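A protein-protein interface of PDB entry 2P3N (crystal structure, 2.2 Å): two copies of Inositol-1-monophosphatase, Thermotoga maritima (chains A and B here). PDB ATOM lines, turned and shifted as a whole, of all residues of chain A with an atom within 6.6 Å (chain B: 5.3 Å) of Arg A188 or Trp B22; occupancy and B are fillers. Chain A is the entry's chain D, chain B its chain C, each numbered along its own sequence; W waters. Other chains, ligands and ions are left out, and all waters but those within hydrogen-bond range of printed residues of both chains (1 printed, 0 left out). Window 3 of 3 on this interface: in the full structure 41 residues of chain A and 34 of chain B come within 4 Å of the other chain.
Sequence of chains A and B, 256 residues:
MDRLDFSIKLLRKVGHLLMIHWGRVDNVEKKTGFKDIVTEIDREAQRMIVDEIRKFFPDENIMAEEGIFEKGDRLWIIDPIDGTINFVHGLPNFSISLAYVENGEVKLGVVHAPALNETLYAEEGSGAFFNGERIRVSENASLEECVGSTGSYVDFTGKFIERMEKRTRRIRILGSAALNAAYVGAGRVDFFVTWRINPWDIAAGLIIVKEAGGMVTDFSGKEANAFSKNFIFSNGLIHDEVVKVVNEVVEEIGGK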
ATOM      1  N   LEU A 116     -20.897 -26.052 -33.519  1.00  0.00           N
ATOM      2  CA  LEU A 116     -19.700 -25.693 -32.763  1.00  0.00           C
ATOM      3  C   LEU A 116     -19.804 -25.975 -31.260  1.00  0.00           C
ATOM      4  O   LEU A 116     -18.785 -25.969 -30.567  1.00  0.00           O
ATOM      5  CB  LEU A 116     -19.359 -24.203 -32.970  1.00  0.00           C
ATOM      6  CG  LEU A 116     -19.203 -23.676 -34.407  1.00  0.00           C
ATOM      7  CD1 LEU A 116     -19.083 -22.181 -34.391  1.00  0.00           C
ATOM      8  CD2 LEU A 116     -18.000 -24.286 -35.070  1.00  0.00           C
ATOM      9  N   GLU A 118     -21.279 -24.055 -29.076  1.00  0.00           N
ATOM     10  CA  GLU A 118     -21.006 -22.791 -28.425  1.00  0.00           C
ATOM     11  C   GLU A 118     -22.267 -22.037 -28.074  1.00  0.00           C
ATOM     12  O   GLU A 118     -23.032 -21.628 -28.946  1.00  0.00           O
ATOM     13  CB  GLU A 118     -20.120 -21.926 -29.326  1.00  0.00           C
ATOM     14  CG  GLU A 118     -18.812 -22.610 -29.718  1.00  0.00           C
ATOM     15  CD  GLU A 118     -17.988 -21.810 -30.699  1.00  0.00           C
ATOM     16  OE1 GLU A 118     -16.817 -22.178 -30.943  1.00  0.00           O
ATOM     17  OE2 GLU A 118     -18.519 -20.811 -31.223  1.00  0.00           O
ATOM     18  N   LEU A 120     -23.216 -18.779 -26.264  1.00  0.00           N
ATOM     19  CA  LEU A 120     -22.792 -17.520 -25.693  1.00  0.00           C
ATOM     20  C   LEU A 120     -24.107 -16.846 -25.330  1.00  0.00           C
ATOM     21  O   LEU A 120     -25.110 -17.036 -26.018  1.00  0.00           O
ATOM     22  CB  LEU A 120     -22.004 -16.705 -26.722  1.00  0.00           C
ATOM     23  CG  LEU A 120     -20.792 -17.467 -27.268  1.00  0.00           C
ATOM     24  CD1 LEU A 120     -21.206 -18.273 -28.491  1.00  0.00           C
ATOM     25  CD2 LEU A 120     -19.698 -16.498 -27.644  1.00  0.00           C
ATOM     26  N   PHE A 130     -20.211 -17.959 -21.662  1.00  0.00           N
ATOM     27  CA  PHE A 130     -19.961 -18.852 -22.777  1.00  0.00           C
ATOM     28  C   PHE A 130     -19.960 -20.223 -22.128  1.00  0.00           C
ATOM     29  O   PHE A 130     -19.027 -20.573 -21.418  1.00  0.00           O
ATOM     30  CB  PHE A 130     -18.599 -18.518 -23.379  1.00  0.00           C
ATOM     31  CG  PHE A 130     -18.299 -19.239 -24.653  1.00  0.00           C
ATOM     32  CD1 PHE A 130     -17.458 -18.670 -25.597  1.00  0.00           C
ATOM     33  CD2 PHE A 130     -18.825 -20.492 -24.907  1.00  0.00           C
ATOM     34  CE1 PHE A 130     -17.145 -19.345 -26.776  1.00  0.00           C
ATOM     35  CE2 PHE A 130     -18.515 -21.170 -26.080  1.00  0.00           C
ATOM     36  CZ  PHE A 130     -17.675 -20.595 -27.014  1.00  0.00           C
ATOM     37  N   ARG A 136     -15.216 -11.654 -21.523  1.00  0.00           N
ATOM     38  CA  ARG A 136     -15.066 -10.202 -21.619  1.00  0.00           C
ATOM     39  C   ARG A 136     -14.371  -9.912 -22.948  1.00  0.00           C
ATOM     40  O   ARG A 136     -13.577 -10.728 -23.418  1.00  0.00           O
ATOM     41  CB  ARG A 136     -14.188  -9.699 -20.468  1.00  0.00           C
ATOM     42  CG  ARG A 136     -14.681 -10.112 -19.093  1.00  0.00           C
ATOM     43  CD  ARG A 136     -13.711  -9.710 -17.982  1.00  0.00           C
ATOM     44  NE  ARG A 136     -14.278  -9.912 -16.644  1.00  0.00           N
ATOM     45  CZ  ARG A 136     -14.496 -11.097 -16.076  1.00  0.00           C
ATOM     46  NH1 ARG A 136     -14.196 -12.227 -16.716  1.00  0.00           N
ATOM     47  NH2 ARG A 136     -15.019 -11.151 -14.857  1.00  0.00           N
ATOM     48  N   VAL A 137     -14.654  -8.756 -23.547  1.00  0.00           N
ATOM     49  CA  VAL A 137     -14.031  -8.389 -24.825  1.00  0.00           C
ATOM     50  C   VAL A 137     -12.489  -8.361 -24.734  1.00  0.00           C
ATOM     51  O   VAL A 137     -11.924  -8.419 -23.638  1.00  0.00           O
ATOM     52  CB  VAL A 137     -14.564  -7.015 -25.323  1.00  0.00           C
ATOM     53  CG1 VAL A 137     -16.073  -7.082 -25.517  1.00  0.00           C
ATOM     54  CG2 VAL A 137     -14.216  -5.922 -24.324  1.00  0.00           C
ATOM     55  N   SER A 138     -11.810  -8.276 -25.879  1.00  0.00           N
ATOM     56  CA  SER A 138     -10.341  -8.278 -25.906  1.00  0.00           C
ATOM     57  C   SER A 138      -9.689  -7.011 -25.367  1.00  0.00           C
ATOM     58  O   SER A 138     -10.351  -5.993 -25.130  1.00  0.00           O
ATOM     59  CB  SER A 138      -9.812  -8.498 -27.327  1.00  0.00           C
ATOM     60  OG  SER A 138      -9.789  -7.275 -28.051  1.00  0.00           O
ATOM     61  N   VAL A 147      -8.090  -8.419 -34.904  1.00  0.00           N
ATOM     62  CA  VAL A 147      -8.664  -9.283 -35.930  1.00  0.00           C
ATOM     63  C   VAL A 147     -10.106  -8.771 -36.058  1.00  0.00           C
ATOM     64  O   VAL A 147     -10.924  -9.012 -35.177  1.00  0.00           O
ATOM     65  CB  VAL A 147      -8.724 -10.789 -35.526  1.00  0.00           C
ATOM     66  CG1 VAL A 147      -9.679 -11.515 -36.455  1.00  0.00           C
ATOM     67  CG2 VAL A 147      -7.340 -11.444 -35.626  1.00  0.00           C
ATOM     68  N   ALA A 182     -21.248 -12.062 -31.128  1.00  0.00           N
ATOM     69  CA  ALA A 182     -21.021 -12.729 -29.861  1.00  0.00           C
ATOM     70  C   ALA A 182     -19.531 -12.981 -29.679  1.00  0.00           C
ATOM     71  O   ALA A 182     -19.034 -13.085 -28.554  1.00  0.00           O
ATOM     72  CB  ALA A 182     -21.788 -14.046 -29.830  1.00  0.00           C
ATOM     73  N   TYR A 183     -18.822 -13.096 -30.796  1.00  0.00           N
ATOM     74  CA  TYR A 183     -17.392 -13.331 -30.763  1.00  0.00           C
ATOM     75  C   TYR A 183     -16.603 -12.123 -30.256  1.00  0.00           C
ATOM     76  O   TYR A 183     -15.555 -12.295 -29.627  1.00  0.00           O
ATOM     77  CB  TYR A 183     -16.919 -13.768 -32.145  1.00  0.00           C
ATOM     78  CG  TYR A 183     -16.987 -15.266 -32.352  1.00  0.00           C
ATOM     79  CD1 TYR A 183     -17.731 -16.087 -31.494  1.00  0.00           C
ATOM     80  CD2 TYR A 183     -16.276 -15.876 -33.384  1.00  0.00           C
ATOM     81  CE1 TYR A 183     -17.755 -17.489 -31.660  1.00  0.00           C
ATOM     82  CE2 TYR A 183     -16.292 -17.273 -33.561  1.00  0.00           C
ATOM     83  CZ  TYR A 183     -17.029 -18.069 -32.698  1.00  0.00           C
ATOM     84  OH  TYR A 183     -17.017 -19.434 -32.885  1.00  0.00           O
ATOM     85  N   VAL A 184     -17.080 -10.904 -30.511  1.00  0.00           N
ATOM     86  CA  VAL A 184     -16.359  -9.749 -29.986  1.00  0.00           C
ATOM     87  C   VAL A 184     -16.508  -9.820 -28.453  1.00  0.00           C
ATOM     88  O   VAL A 184     -15.546  -9.593 -27.712  1.00  0.00           O
ATOM     89  CB  VAL A 184     -16.912  -8.384 -30.518  1.00  0.00           C
ATOM     90  CG1 VAL A 184     -16.990  -8.391 -32.036  1.00  0.00           C
ATOM     91  CG2 VAL A 184     -18.258  -8.098 -29.931  1.00  0.00           C
ATOM     92  N   GLY A 185     -17.712 -10.160 -27.988  1.00  0.00           N
ATOM     93  CA  GLY A 185     -17.952 -10.279 -26.564  1.00  0.00           C
ATOM     94  C   GLY A 185     -17.084 -11.372 -25.961  1.00  0.00           C
ATOM     95  O   GLY A 185     -16.620 -11.261 -24.821  1.00  0.00           O
ATOM     96  N   ALA A 186     -16.862 -12.437 -26.730  1.00  0.00           N
ATOM     97  CA  ALA A 186     -16.042 -13.558 -26.271  1.00  0.00           C
ATOM     98  C   ALA A 186     -14.578 -13.186 -26.353  1.00  0.00           C
ATOM     99  O   ALA A 186     -13.721 -13.860 -25.780  1.00  0.00           O
ATOM    100  CB  ALA A 186     -16.309 -14.791 -27.114  1.00  0.00           C
ATOM    101  N   GLY A 187     -14.298 -12.112 -27.083  1.00  0.00           N
ATOM    102  CA  GLY A 187     -12.931 -11.657 -27.219  1.00  0.00           C
ATOM    103  C   GLY A 187     -12.144 -12.448 -28.236  1.00  0.00           C
ATOM    104  O   GLY A 187     -10.919 -12.373 -28.263  1.00  0.00           O
ATOM    105  N   ARG A 188     -12.842 -13.205 -29.076  1.00  0.00           N
ATOM    106  CA  ARG A 188     -12.190 -14.004 -30.108  1.00  0.00           C
ATOM    107  C   ARG A 188     -11.903 -13.129 -31.324  1.00  0.00           C
ATOM    108  O   ARG A 188     -11.058 -13.456 -32.169  1.00  0.00           O
ATOM    109  CB  ARG A 188     -13.079 -15.175 -30.505  1.00  0.00           C
ATOM    110  CG  ARG A 188     -13.227 -16.191 -29.417  1.00  0.00           C
ATOM    111  CD  ARG A 188     -14.232 -17.219 -29.817  1.00  0.00           C
ATOM    112  NE  ARG A 188     -14.226 -18.363 -28.913  1.00  0.00           N
ATOM    113  CZ  ARG A 188     -14.690 -19.560 -29.244  1.00  0.00           C
ATOM    114  NH1 ARG A 188     -15.193 -19.750 -30.457  1.00  0.00           N
ATOM    115  NH2 ARG A 188     -14.628 -20.566 -28.376  1.00  0.00           N
ATOM    116  N   VAL A 189     -12.612 -12.009 -31.384  1.00  0.00           N
ATOM    117  CA  VAL A 189     -12.462 -11.039 -32.450  1.00  0.00           C
ATOM    118  C   VAL A 189     -12.524  -9.661 -31.787  1.00  0.00           C
ATOM    119  O   VAL A 189     -13.184  -9.491 -30.763  1.00  0.00           O
ATOM    120  CB  VAL A 189     -13.581 -11.232 -33.511  1.00  0.00           C
ATOM    121  CG1 VAL A 189     -14.279  -9.903 -33.837  1.00  0.00           C
ATOM    122  CG2 VAL A 189     -12.972 -11.864 -34.769  1.00  0.00           C
ATOM    123  N   ASP A 190     -11.843  -8.679 -32.370  1.00  0.00           N
ATOM    124  CA  ASP A 190     -11.799  -7.348 -31.780  1.00  0.00           C
ATOM    125  C   ASP A 190     -12.890  -6.366 -32.202  1.00  0.00           C
ATOM    126  O   ASP A 190     -13.218  -5.437 -31.467  1.00  0.00           O
ATOM    127  CB  ASP A 190     -10.396  -6.795 -31.985  1.00  0.00           C
ATOM    128  CG  ASP A 190      -9.337  -7.735 -31.409  1.00  0.00           C
ATOM    129  OD1 ASP A 190      -9.387  -8.012 -30.191  1.00  0.00           O
ATOM    130  OD2 ASP A 190      -8.465  -8.218 -32.164  1.00  0.00           O
ATOM    131  N   LEU B  18      -2.568 -28.450 -28.402  1.00  0.00           N
ATOM    132  CA  LEU B  18      -3.006 -27.147 -28.885  1.00  0.00           C
ATOM    133  C   LEU B  18      -4.196 -26.605 -28.099  1.00  0.00           C
ATOM    134  O   LEU B  18      -4.270 -25.403 -27.816  1.00  0.00           O
ATOM    135  CB  LEU B  18      -3.369 -27.206 -30.383  1.00  0.00           C
ATOM    136  CG  LEU B  18      -2.239 -27.473 -31.382  1.00  0.00           C
ATOM    137  CD1 LEU B  18      -2.779 -27.312 -32.802  1.00  0.00           C
ATOM    138  CD2 LEU B  18      -1.088 -26.507 -31.144  1.00  0.00           C
ATOM    139  N   MET B  19      -5.125 -27.495 -27.755  1.00  0.00           N
ATOM    140  CA  MET B  19      -6.320 -27.106 -27.020  1.00  0.00           C
ATOM    141  C   MET B  19      -5.991 -26.490 -25.670  1.00  0.00           C
ATOM    142  O   MET B  19      -6.747 -25.659 -25.154  1.00  0.00           O
ATOM    143  CB  MET B  19      -7.241 -28.310 -26.841  1.00  0.00           C
ATOM    144  CG  MET B  19      -7.935 -28.745 -28.124  1.00  0.00           C
ATOM    145  SD  MET B  19      -8.770 -27.376 -28.955  1.00  0.00           S
ATOM    146  CE  MET B  19     -10.119 -27.032 -27.827  1.00  0.00           C
ATOM    147  N   ILE B  20      -4.861 -26.895 -25.098  1.00  0.00           N
ATOM    148  CA  ILE B  20      -4.428 -26.349 -23.820  1.00  0.00           C
ATOM    149  C   ILE B  20      -4.141 -24.846 -23.933  1.00  0.00           C
ATOM    150  O   ILE B  20      -4.535 -24.061 -23.065  1.00  0.00           O
ATOM    151  CB  ILE B  20      -3.143 -27.019 -23.337  1.00  0.00           C
ATOM    152  CG1 ILE B  20      -3.319 -28.532 -23.311  1.00  0.00           C
ATOM    153  CG2 ILE B  20      -2.793 -26.505 -21.954  1.00  0.00           C
ATOM    154  CD1 ILE B  20      -2.101 -29.279 -22.812  1.00  0.00           C
ATOM    155  N   HIS B  21      -3.462 -24.445 -25.007  1.00  0.00           N
ATOM    156  CA  HIS B  21      -3.110 -23.045 -25.198  1.00  0.00           C
ATOM    157  C   HIS B  21      -3.968 -22.272 -26.186  1.00  0.00           C
ATOM    158  O   HIS B  21      -3.686 -21.104 -26.455  1.00  0.00           O
ATOM    159  CB  HIS B  21      -1.652 -22.932 -25.626  1.00  0.00           C
ATOM    160  CG  HIS B  21      -0.700 -23.646 -24.721  1.00  0.00           C
ATOM    161  ND1 HIS B  21      -0.460 -25.001 -24.813  1.00  0.00           N
ATOM    162  CD2 HIS B  21       0.057 -23.199 -23.690  1.00  0.00           C
ATOM    163  CE1 HIS B  21       0.404 -25.356 -23.877  1.00  0.00           C
ATOM    164  NE2 HIS B  21       0.732 -24.280 -23.182  1.00  0.00           N
ATOM    165  N   TRP B  22      -4.999 -22.910 -26.734  1.00  0.00           N
ATOM    166  CA  TRP B  22      -5.888 -22.243 -27.680  1.00  0.00           C
ATOM    167  C   TRP B  22      -6.457 -20.982 -27.031  1.00  0.00           C
ATOM    168  O   TRP B  22      -7.171 -21.054 -26.025  1.00  0.00           O
ATOM    169  CB  TRP B  22      -7.031 -23.187 -28.108  1.00  0.00           C
ATOM    170  CG  TRP B  22      -7.985 -22.567 -29.090  1.00  0.00           C
ATOM    171  CD1 TRP B  22      -7.676 -21.676 -30.080  1.00  0.00           C
ATOM    172  CD2 TRP B  22      -9.407 -22.733 -29.138  1.00  0.00           C
ATOM    173  NE1 TRP B  22      -8.816 -21.269 -30.731  1.00  0.00           N
ATOM    174  CE2 TRP B  22      -9.892 -21.901 -30.170  1.00  0.00           C
ATOM    175  CE3 TRP B  22     -10.317 -23.497 -28.406  1.00  0.00           C
ATOM    176  CZ2 TRP B  22     -11.251 -21.813 -30.486  1.00  0.00           C
ATOM    177  CZ3 TRP B  22     -11.665 -23.407 -28.719  1.00  0.00           C
ATOM    178  CH2 TRP B  22     -12.119 -22.568 -29.750  1.00  0.00           C
ATOM    179  N   GLY B  23      -6.127 -19.824 -27.599  1.00  0.00           N
ATOM    180  CA  GLY B  23      -6.618 -18.572 -27.052  1.00  0.00           C
ATOM    181  C   GLY B  23      -5.916 -18.108 -25.782  1.00  0.00           C
ATOM    182  O   GLY B  23      -6.124 -16.980 -25.359  1.00  0.00           O
ATOM    183  N   ARG B  24      -5.084 -18.959 -25.184  1.00  0.00           N
ATOM    184  CA  ARG B  24      -4.383 -18.622 -23.953  1.00  0.00           C
ATOM    185  C   ARG B  24      -2.878 -18.540 -24.179  1.00  0.00           C
ATOM    186  O   ARG B  24      -2.093 -19.110 -23.414  1.00  0.00           O
ATOM    187  CB  ARG B  24      -4.650 -19.680 -22.879  1.00  0.00           C
ATOM    188  CG  ARG B  24      -6.005 -20.369 -22.956  1.00  0.00           C
ATOM    189  CD  ARG B  24      -7.061 -19.793 -22.009  1.00  0.00           C
ATOM    190  NE  ARG B  24      -7.464 -18.419 -22.316  1.00  0.00           N
ATOM    191  CZ  ARG B  24      -8.628 -17.880 -21.944  1.00  0.00           C
ATOM    192  NH1 ARG B  24      -8.914 -16.620 -22.259  1.00  0.00           N
ATOM    193  NH2 ARG B  24      -9.519 -18.602 -21.268  1.00  0.00           N
ATOM    194  N   ASN B  86      -5.571 -17.146 -35.793  1.00  0.00           N
ATOM    195  CA  ASN B  86      -6.854 -17.624 -35.276  1.00  0.00           C
ATOM    196  C   ASN B  86      -6.634 -18.284 -33.919  1.00  0.00           C
ATOM    197  O   ASN B  86      -7.326 -17.975 -32.939  1.00  0.00           O
ATOM    198  CB  ASN B  86      -7.451 -18.662 -36.230  1.00  0.00           C
ATOM    199  CG  ASN B  86      -8.334 -18.046 -37.275  1.00  0.00           C
ATOM    200  OD1 ASN B  86      -8.362 -16.833 -37.433  1.00  0.00           O
ATOM    201  ND2 ASN B  86      -9.065 -18.875 -38.000  1.00  0.00           N
ATOM    202  N   PHE B  87      -5.661 -19.192 -33.880  1.00  0.00           N
ATOM    203  CA  PHE B  87      -5.308 -19.948 -32.683  1.00  0.00           C
ATOM    204  C   PHE B  87      -4.976 -19.046 -31.496  1.00  0.00           C
ATOM    205  O   PHE B  87      -5.330 -19.350 -30.354  1.00  0.00           O
ATOM    206  CB  PHE B  87      -4.127 -20.858 -33.003  1.00  0.00           C
ATOM    207  CG  PHE B  87      -3.629 -21.638 -31.833  1.00  0.00           C
ATOM    208  CD1 PHE B  87      -4.276 -22.784 -31.425  1.00  0.00           C
ATOM    209  CD2 PHE B  87      -2.517 -21.206 -31.119  1.00  0.00           C
ATOM    210  CE1 PHE B  87      -3.825 -23.496 -30.317  1.00  0.00           C
ATOM    211  CE2 PHE B  87      -2.064 -21.909 -30.014  1.00  0.00           C
ATOM    212  CZ  PHE B  87      -2.719 -23.056 -29.612  1.00  0.00           C
ATOM    213  N   HIS B  89      -5.927 -15.686 -31.174  1.00  0.00           N
ATOM    214  CA  HIS B  89      -7.106 -14.913 -30.819  1.00  0.00           C
ATOM    215  C   HIS B  89      -8.248 -15.709 -30.207  1.00  0.00           C
ATOM    216  O   HIS B  89      -9.120 -15.131 -29.546  1.00  0.00           O
ATOM    217  CB  HIS B  89      -7.595 -14.134 -32.042  1.00  0.00           C
ATOM    218  CG  HIS B  89      -6.812 -12.882 -32.285  1.00  0.00           C
ATOM    219  ND1 HIS B  89      -7.300 -11.629 -31.981  1.00  0.00           N
ATOM    220  CD2 HIS B  89      -5.538 -12.699 -32.700  1.00  0.00           C
ATOM    221  CE1 HIS B  89      -6.359 -10.728 -32.196  1.00  0.00           C
ATOM    222  NE2 HIS B  89      -5.280 -11.352 -32.632  1.00  0.00           N
ATOM    223  N   GLY B  90      -8.251 -17.024 -30.421  1.00  0.00           N
ATOM    224  CA  GLY B  90      -9.303 -17.859 -29.858  1.00  0.00           C
ATOM    225  C   GLY B  90     -10.342 -18.371 -30.839  1.00  0.00           C
ATOM    226  O   GLY B  90     -11.344 -18.948 -30.427  1.00  0.00           O
ATOM    227  N   LEU B  91     -10.123 -18.142 -32.133  1.00  0.00           N
ATOM    228  CA  LEU B  91     -11.056 -18.629 -33.144  1.00  0.00           C
ATOM    229  C   LEU B  91     -10.759 -20.108 -33.416  1.00  0.00           C
ATOM    230  O   LEU B  91      -9.601 -20.549 -33.418  1.00  0.00           O
ATOM    231  CB  LEU B  91     -10.966 -17.793 -34.421  1.00  0.00           C
ATOM    232  CG  LEU B  91     -11.616 -16.424 -34.206  1.00  0.00           C
ATOM    233  CD1 LEU B  91     -11.305 -15.486 -35.367  1.00  0.00           C
ATOM    234  CD2 LEU B  91     -13.122 -16.613 -34.040  1.00  0.00           C
ATOM    235  N   PRO B  92     -11.816 -20.895 -33.639  1.00  0.00           N
ATOM    236  CA  PRO B  92     -11.718 -22.332 -33.894  1.00  0.00           C
ATOM    237  C   PRO B  92     -11.112 -22.812 -35.211  1.00  0.00           C
ATOM    238  O   PRO B  92     -10.676 -23.971 -35.318  1.00  0.00           O
ATOM    239  CB  PRO B  92     -13.160 -22.799 -33.688  1.00  0.00           C
ATOM    240  CG  PRO B  92     -13.953 -21.643 -34.198  1.00  0.00           C
ATOM    241  CD  PRO B  92     -13.225 -20.449 -33.638  1.00  0.00           C
ATOM    242  N   PHE B  94      -8.403 -23.337 -36.978  1.00  0.00           N
ATOM    243  CA  PHE B  94      -6.960 -23.510 -36.976  1.00  0.00           C
ATOM    244  C   PHE B  94      -6.778 -25.019 -37.077  1.00  0.00           C
ATOM    245  O   PHE B  94      -7.613 -25.780 -36.597  1.00  0.00           O
ATOM    246  CB  PHE B  94      -6.320 -22.920 -35.706  1.00  0.00           C
ATOM    247  CG  PHE B  94      -6.658 -23.651 -34.441  1.00  0.00           C
ATOM    248  CD1 PHE B  94      -5.943 -24.782 -34.062  1.00  0.00           C
ATOM    249  CD2 PHE B  94      -7.708 -23.215 -33.631  1.00  0.00           C
ATOM    250  CE1 PHE B  94      -6.272 -25.475 -32.888  1.00  0.00           C
ATOM    251  CE2 PHE B  94      -8.046 -23.897 -32.459  1.00  0.00           C
ATOM    252  CZ  PHE B  94      -7.332 -25.028 -32.086  1.00  0.00           C
ATOM    253  N   ALA B 115     -10.328 -27.824 -32.286  1.00  0.00           N
ATOM    254  CA  ALA B 115     -11.441 -27.144 -31.661  1.00  0.00           C
ATOM    255  C   ALA B 115     -12.704 -27.580 -32.328  1.00  0.00           C
ATOM    256  O   ALA B 115     -13.761 -27.594 -31.704  1.00  0.00           O
ATOM    257  CB  ALA B 115     -11.289 -25.652 -31.784  1.00  0.00           C
HETATM  258  O   HOH W   1      -9.391 -10.922 -30.209  1.00  0.00           O
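O of Gly B90 is in hydrogen-bond range of NE of Arg A188, at 3.3 Å.
The backbone carbonyl oxygen of Tyr A183 sits at hydrogen-bond distance from the backbone NH of Arg A188.
The indole nitrogen of Trp B22 sits close to the backbone carbonyl oxygen of Gly B90, at 3.4 Å.
The side-chain carboxylate of Glu A118 is in salt-bridge range of the guanidinium group of Arg A188, at 3.0 Å.
The side-chain carboxylate (OD2) of Asp A190 is in hydrogen-bond range of the backbone NH (N) of Val A147 (2.8 Å).
The backbone carbonyl oxygen of Asn B86 is in hydrogen-bond range of the backbone NH of Leu B91 (2.9 Å).
O of Tyr A183 lies within hydrogen-bond range of N of Val A189 (3.4 Å).
His B89 touches Val A147 (NE2 to CG2, 3.6 Å).
CE2 of Tyr A183 touches CD2 of Leu B91, at 3.3 Å.
Pro B92 touches Tyr A183 (CD to OH, 3.997 Å).
Gly A187 touches His B89 (O to O, 3.5 Å).
NH2 of Arg A188 touches CH2 of Trp B22 (3.5 Å).
Arg A188 touches His B89 (CA to O, 3.3 Å).
Leu B91 touches Arg A188.
NH1 of Arg A188 touches CD of Pro B92, 3.8 Å away.
His B89 touches Asp A190.
Of the printed residues of chain B, Arg A188 touches Trp B22, His B89, Gly B90, Leu B91 and Pro B92.
Trp B22 touches just one residue of chain A: Arg A188.
Printed residues of chain A within 4 Å of Leu B91: Tyr A183 (3.3 Å) and Arg A188 (3.6 Å).
Printed residues of chain B within 4 Å of Val A147: His B89 (3.6 Å).
Of the printed residues of chain B, Tyr A183 touches Leu B91 (3.3 Å) and Pro B92 (3.997 Å).
Val A189 touches none of the printed residues of chain B.
Hydrophobic or aromatic side chains of chain A that line the printed part of chain B: Val A147 and Tyr A183.
Along chain A the printed residues that touch a printed residue of chain B span positions 147 to 190.
Along chain B the printed residues that touch a printed residue of chain A span positions 22 to 92.
Among the printed residues, 10 pairs touch across the chains.
Among the printed residues, no Asp or Glu carboxylate lies within 4 Å of a Lys or Arg side-chain nitrogen of the other chain.
No position is printed for both chains.
Of the 10 pairs that touch across the chains among the printed residues, none has its exchanged pair printed and touching as well.
Water W1 lies within hydrogen-bond range of a ring nitrogen (ND1) of His B89 (2.8 Å), the backbone carbonyl oxygen of Gly A187 (2.9 Å) and the side-chain carboxylate of Asp A190 (2.9 Å).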
